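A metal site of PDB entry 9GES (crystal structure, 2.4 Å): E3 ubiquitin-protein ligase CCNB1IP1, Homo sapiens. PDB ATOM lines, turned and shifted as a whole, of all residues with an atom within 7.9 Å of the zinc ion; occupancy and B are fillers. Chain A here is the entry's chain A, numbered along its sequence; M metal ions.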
ATOM      1  N   LEU A  11      -4.066 -11.689  -2.111  1.00  0.00           N
ATOM      2  CA  LEU A  11      -5.131 -12.676  -2.134  1.00  0.00           C
ATOM      3  C   LEU A  11      -4.531 -14.068  -2.167  1.00  0.00           C
ATOM      4  O   LEU A  11      -3.425 -14.275  -2.665  1.00  0.00           O
ATOM      5  CB  LEU A  11      -6.054 -12.482  -3.343  1.00  0.00           C
ATOM      6  CG  LEU A  11      -6.751 -11.119  -3.478  1.00  0.00           C
ATOM      7  CD1 LEU A  11      -7.609 -11.080  -4.723  1.00  0.00           C
ATOM      8  CD2 LEU A  11      -7.585 -10.817  -2.237  1.00  0.00           C
ATOM      9  N   CYS A  12      -5.277 -15.025  -1.607  1.00  0.00           N
ATOM     10  CA  CYS A  12      -4.842 -16.415  -1.633  1.00  0.00           C
ATOM     11  C   CYS A  12      -4.714 -16.893  -3.076  1.00  0.00           C
ATOM     12  O   CYS A  12      -5.604 -16.678  -3.897  1.00  0.00           O
ATOM     13  CB  CYS A  12      -5.838 -17.297  -0.871  1.00  0.00           C
ATOM     14  SG  CYS A  12      -5.436 -19.052  -0.800  1.00  0.00           S
ATOM     15  N   ASN A  13      -3.587 -17.546  -3.386  1.00  0.00           N
ATOM     16  CA  ASN A  13      -3.352 -18.032  -4.735  1.00  0.00           C
ATOM     17  C   ASN A  13      -4.022 -19.373  -5.005  1.00  0.00           C
ATOM     18  O   ASN A  13      -3.929 -19.872  -6.129  1.00  0.00           O
ATOM     19  CB  ASN A  13      -1.851 -18.122  -5.017  1.00  0.00           C
ATOM     20  CG  ASN A  13      -1.187 -16.765  -5.164  1.00  0.00           C
ATOM     21  OD1 ASN A  13      -0.104 -16.519  -4.640  1.00  0.00           O
ATOM     22  ND2 ASN A  13      -1.858 -15.864  -5.881  1.00  0.00           N
ATOM     23  N   TYR A  14      -4.669 -19.963  -4.003  1.00  0.00           N
ATOM     24  CA  TYR A  14      -5.520 -21.121  -4.260  1.00  0.00           C
ATOM     25  C   TYR A  14      -6.759 -20.671  -5.021  1.00  0.00           C
ATOM     26  O   TYR A  14      -7.403 -19.690  -4.638  1.00  0.00           O
ATOM     27  CB  TYR A  14      -5.900 -21.783  -2.935  1.00  0.00           C
ATOM     28  CG  TYR A  14      -6.496 -23.165  -3.076  1.00  0.00           C
ATOM     29  CD1 TYR A  14      -5.695 -24.297  -3.145  1.00  0.00           C
ATOM     30  CD2 TYR A  14      -7.877 -23.351  -3.114  1.00  0.00           C
ATOM     31  CE1 TYR A  14      -6.240 -25.563  -3.266  1.00  0.00           C
ATOM     32  CE2 TYR A  14      -8.431 -24.605  -3.235  1.00  0.00           C
ATOM     33  CZ  TYR A  14      -7.605 -25.711  -3.312  1.00  0.00           C
ATOM     34  OH  TYR A  14      -8.158 -26.965  -3.433  1.00  0.00           O
ATOM     35  N   ARG A  15      -7.079 -21.383  -6.100  1.00  0.00           N
ATOM     36  CA  ARG A  15      -8.133 -20.921  -7.010  1.00  0.00           C
ATOM     37  C   ARG A  15      -9.488 -20.841  -6.333  1.00  0.00           C
ATOM     38  O   ARG A  15     -10.299 -19.976  -6.685  1.00  0.00           O
ATOM     39  CB  ARG A  15      -8.209 -21.834  -8.230  1.00  0.00           C
ATOM     40  CG  ARG A  15      -6.944 -21.859  -9.077  1.00  0.00           C
ATOM     41  CD  ARG A  15      -7.134 -22.707 -10.326  1.00  0.00           C
ATOM     42  NE  ARG A  15      -5.947 -22.727 -11.160  1.00  0.00           N
ATOM     43  CZ  ARG A  15      -5.858 -23.353 -12.329  1.00  0.00           C
ATOM     44  NH1 ARG A  15      -6.884 -24.020 -12.830  1.00  0.00           N
ATOM     45  NH2 ARG A  15      -4.719 -23.301 -13.010  1.00  0.00           N
ATOM     46  N   LYS A  16      -9.753 -21.713  -5.360  1.00  0.00           N
ATOM     47  CA  LYS A  16     -11.067 -21.770  -4.723  1.00  0.00           C
ATOM     48  C   LYS A  16     -11.173 -20.893  -3.487  1.00  0.00           C
ATOM     49  O   LYS A  16     -12.227 -20.866  -2.852  1.00  0.00           O
ATOM     50  CB  LYS A  16     -11.409 -23.222  -4.355  1.00  0.00           C
ATOM     51  CG  LYS A  16     -11.302 -24.185  -5.518  1.00  0.00           C
ATOM     52  CD  LYS A  16     -11.475 -25.617  -5.060  1.00  0.00           C
ATOM     53  CE  LYS A  16     -11.315 -26.602  -6.218  1.00  0.00           C
ATOM     54  NZ  LYS A  16     -11.457 -28.012  -5.775  1.00  0.00           N
ATOM     55  N   CYS A  17     -10.116 -20.161  -3.121  1.00  0.00           N
ATOM     56  CA  CYS A  17     -10.132 -19.324  -1.926  1.00  0.00           C
ATOM     57  C   CYS A  17     -10.046 -17.840  -2.257  1.00  0.00           C
ATOM     58  O   CYS A  17     -10.983 -17.092  -1.961  1.00  0.00           O
ATOM     59  CB  CYS A  17      -8.981 -19.724  -1.008  1.00  0.00           C
ATOM     60  SG  CYS A  17      -8.998 -18.987   0.636  1.00  0.00           S
ATOM     61  N   ARG A  18      -8.965 -17.419  -2.911  1.00  0.00           N
ATOM     62  CA  ARG A  18      -8.717 -16.026  -3.300  1.00  0.00           C
ATOM     63  C   ARG A  18      -9.226 -15.036  -2.255  1.00  0.00           C
ATOM     64  O   ARG A  18      -9.933 -14.076  -2.552  1.00  0.00           O
ATOM     65  CB  ARG A  18      -9.327 -15.729  -4.673  1.00  0.00           C
ATOM     66  CG  ARG A  18      -8.723 -16.564  -5.790  1.00  0.00           C
ATOM     67  CD  ARG A  18      -9.188 -16.108  -7.155  1.00  0.00           C
ATOM     68  NE  ARG A  18      -8.820 -14.723  -7.423  1.00  0.00           N
ATOM     69  CZ  ARG A  18      -7.653 -14.351  -7.932  1.00  0.00           C
ATOM     70  NH1 ARG A  18      -6.714 -15.237  -8.242  1.00  0.00           N
ATOM     71  NH2 ARG A  18      -7.427 -13.060  -8.153  1.00  0.00           N
ATOM     72  N   ILE A  19      -8.841 -15.271  -1.003  1.00  0.00           N
ATOM     73  CA  ILE A  19      -9.257 -14.439   0.114  1.00  0.00           C
ATOM     74  C   ILE A  19      -8.134 -13.466   0.449  1.00  0.00           C
ATOM     75  O   ILE A  19      -6.948 -13.741   0.243  1.00  0.00           O
ATOM     76  CB  ILE A  19      -9.643 -15.290   1.356  1.00  0.00           C
ATOM     77  CG1 ILE A  19     -10.477 -14.467   2.333  1.00  0.00           C
ATOM     78  CG2 ILE A  19      -8.395 -15.832   2.045  1.00  0.00           C
ATOM     79  CD1 ILE A  19     -10.825 -15.193   3.608  1.00  0.00           C
ATOM     80  N   LEU A  21      -5.378 -11.673   2.424  1.00  0.00           N
ATOM     81  CA  LEU A  21      -4.418 -12.309   3.325  1.00  0.00           C
ATOM     82  C   LEU A  21      -4.029 -11.335   4.441  1.00  0.00           C
ATOM     83  O   LEU A  21      -3.549 -10.227   4.170  1.00  0.00           O
ATOM     84  CB  LEU A  21      -3.172 -12.758   2.552  1.00  0.00           C
ATOM     85  CG  LEU A  21      -3.435 -13.693   1.365  1.00  0.00           C
ATOM     86  CD1 LEU A  21      -2.125 -14.111   0.741  1.00  0.00           C
ATOM     87  CD2 LEU A  21      -4.251 -14.903   1.792  1.00  0.00           C
ATOM     88  N   ILE A  33       1.606 -17.007  -2.935  1.00  0.00           N
ATOM     89  CA  ILE A  33       1.303 -16.815  -1.522  1.00  0.00           C
ATOM     90  C   ILE A  33      -0.097 -17.351  -1.241  1.00  0.00           C
ATOM     91  O   ILE A  33      -1.017 -17.175  -2.051  1.00  0.00           O
ATOM     92  CB  ILE A  33       1.439 -15.336  -1.107  1.00  0.00           C
ATOM     93  CG1 ILE A  33       1.298 -15.181   0.411  1.00  0.00           C
ATOM     94  CG2 ILE A  33       0.444 -14.461  -1.859  1.00  0.00           C
ATOM     95  CD1 ILE A  33       1.601 -13.780   0.902  1.00  0.00           C
ATOM     96  N   PHE A  34      -0.262 -18.015  -0.106  1.00  0.00           N
ATOM     97  CA  PHE A  34      -1.514 -18.671   0.243  1.00  0.00           C
ATOM     98  C   PHE A  34      -1.892 -18.322   1.681  1.00  0.00           C
ATOM     99  O   PHE A  34      -1.056 -17.911   2.488  1.00  0.00           O
ATOM    100  CB  PHE A  34      -1.410 -20.199   0.092  1.00  0.00           C
ATOM    101  CG  PHE A  34      -1.029 -20.640  -1.297  1.00  0.00           C
ATOM    102  CD1 PHE A  34       0.297 -20.789  -1.650  1.00  0.00           C
ATOM    103  CD2 PHE A  34      -2.001 -20.899  -2.244  1.00  0.00           C
ATOM    104  CE1 PHE A  34       0.655 -21.185  -2.923  1.00  0.00           C
ATOM    105  CE2 PHE A  34      -1.659 -21.305  -3.525  1.00  0.00           C
ATOM    106  CZ  PHE A  34      -0.331 -21.445  -3.867  1.00  0.00           C
ATOM    107  N   CYS A  35      -3.185 -18.491   1.981  1.00  0.00           N
ATOM    108  CA  CYS A  35      -3.672 -18.198   3.317  1.00  0.00           C
ATOM    109  C   CYS A  35      -3.135 -19.202   4.325  1.00  0.00           C
ATOM    110  O   CYS A  35      -2.500 -20.205   3.965  1.00  0.00           O
ATOM    111  CB  CYS A  35      -5.205 -18.196   3.334  1.00  0.00           C
ATOM    112  SG  CYS A  35      -5.970 -19.783   2.947  1.00  0.00           S
ATOM    113  N   ASP A  36      -3.394 -18.926   5.603  1.00  0.00           N
ATOM    114  CA  ASP A  36      -2.866 -19.778   6.672  1.00  0.00           C
ATOM    115  C   ASP A  36      -3.458 -21.183   6.611  1.00  0.00           C
ATOM    116  O   ASP A  36      -2.731 -22.173   6.779  1.00  0.00           O
ATOM    117  CB  ASP A  36      -3.135 -19.142   8.029  1.00  0.00           C
ATOM    118  CG  ASP A  36      -2.177 -19.619   9.102  1.00  0.00           C
ATOM    119  OD1 ASP A  36      -1.245 -20.379   8.780  1.00  0.00           O
ATOM    120  OD2 ASP A  36      -2.360 -19.228  10.271  1.00  0.00           O
ATOM    121  N   GLN A  37      -4.764 -21.299   6.371  1.00  0.00           N
ATOM    122  CA  GLN A  37      -5.412 -22.612   6.366  1.00  0.00           C
ATOM    123  C   GLN A  37      -4.929 -23.457   5.185  1.00  0.00           C
ATOM    124  O   GLN A  37      -4.539 -24.614   5.364  1.00  0.00           O
ATOM    125  CB  GLN A  37      -6.928 -22.449   6.325  1.00  0.00           C
ATOM    126  CG  GLN A  37      -7.479 -21.540   7.414  1.00  0.00           C
ATOM    127  CD  GLN A  37      -7.137 -22.016   8.811  1.00  0.00           C
ATOM    128  OE1 GLN A  37      -7.122 -23.218   9.086  1.00  0.00           O
ATOM    129  NE2 GLN A  37      -6.839 -21.077   9.706  1.00  0.00           N
ATOM    130  N   HIS A  38      -4.957 -22.900   3.977  1.00  0.00           N
ATOM    131  CA  HIS A  38      -4.526 -23.643   2.802  1.00  0.00           C
ATOM    132  C   HIS A  38      -3.019 -23.874   2.802  1.00  0.00           C
ATOM    133  O   HIS A  38      -2.550 -24.938   2.381  1.00  0.00           O
ATOM    134  CB  HIS A  38      -4.966 -22.922   1.534  1.00  0.00           C
ATOM    135  CG  HIS A  38      -6.419 -23.111   1.214  1.00  0.00           C
ATOM    136  ND1 HIS A  38      -7.152 -22.167   0.532  1.00  0.00           N
ATOM    137  CD2 HIS A  38      -7.263 -24.126   1.486  1.00  0.00           C
ATOM    138  CE1 HIS A  38      -8.400 -22.598   0.400  1.00  0.00           C
ATOM    139  NE2 HIS A  38      -8.487 -23.783   0.964  1.00  0.00           N
ATOM    140  N   GLY A  39      -2.247 -22.876   3.241  1.00  0.00           N
ATOM    141  CA  GLY A  39      -0.802 -23.038   3.289  1.00  0.00           C
ATOM    142  C   GLY A  39      -0.366 -24.106   4.272  1.00  0.00           C
ATOM    143  O   GLY A  39       0.517 -24.920   3.967  1.00  0.00           O
HETATM  144 ZN    ZN M   1      -6.875 -20.124   0.793  1.00  0.00          ZN
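Along chain A the residues within 4 Å of the zinc ion span positions 12 to 38.
The nearest printed residue that does not touch the zinc ion is Tyr 14 (4.2 Å).
A ring nitrogen (ND1) of His 38 binds the zinc ion (2.1 Å).
The side-chain sulfur (SG) of Cys 35 is bound to the zinc ion (2.4 Å).
The zinc ion is bound by SG of Cys 12.
SG of Cys 17 binds the zinc ion (2.4 Å).
N of Tyr 14 lies close to SG of Cys 12, 3.4 Å away.
N of Cys 12 is in hydrogen-bond range of O of Ile 19, at 2.8 Å.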
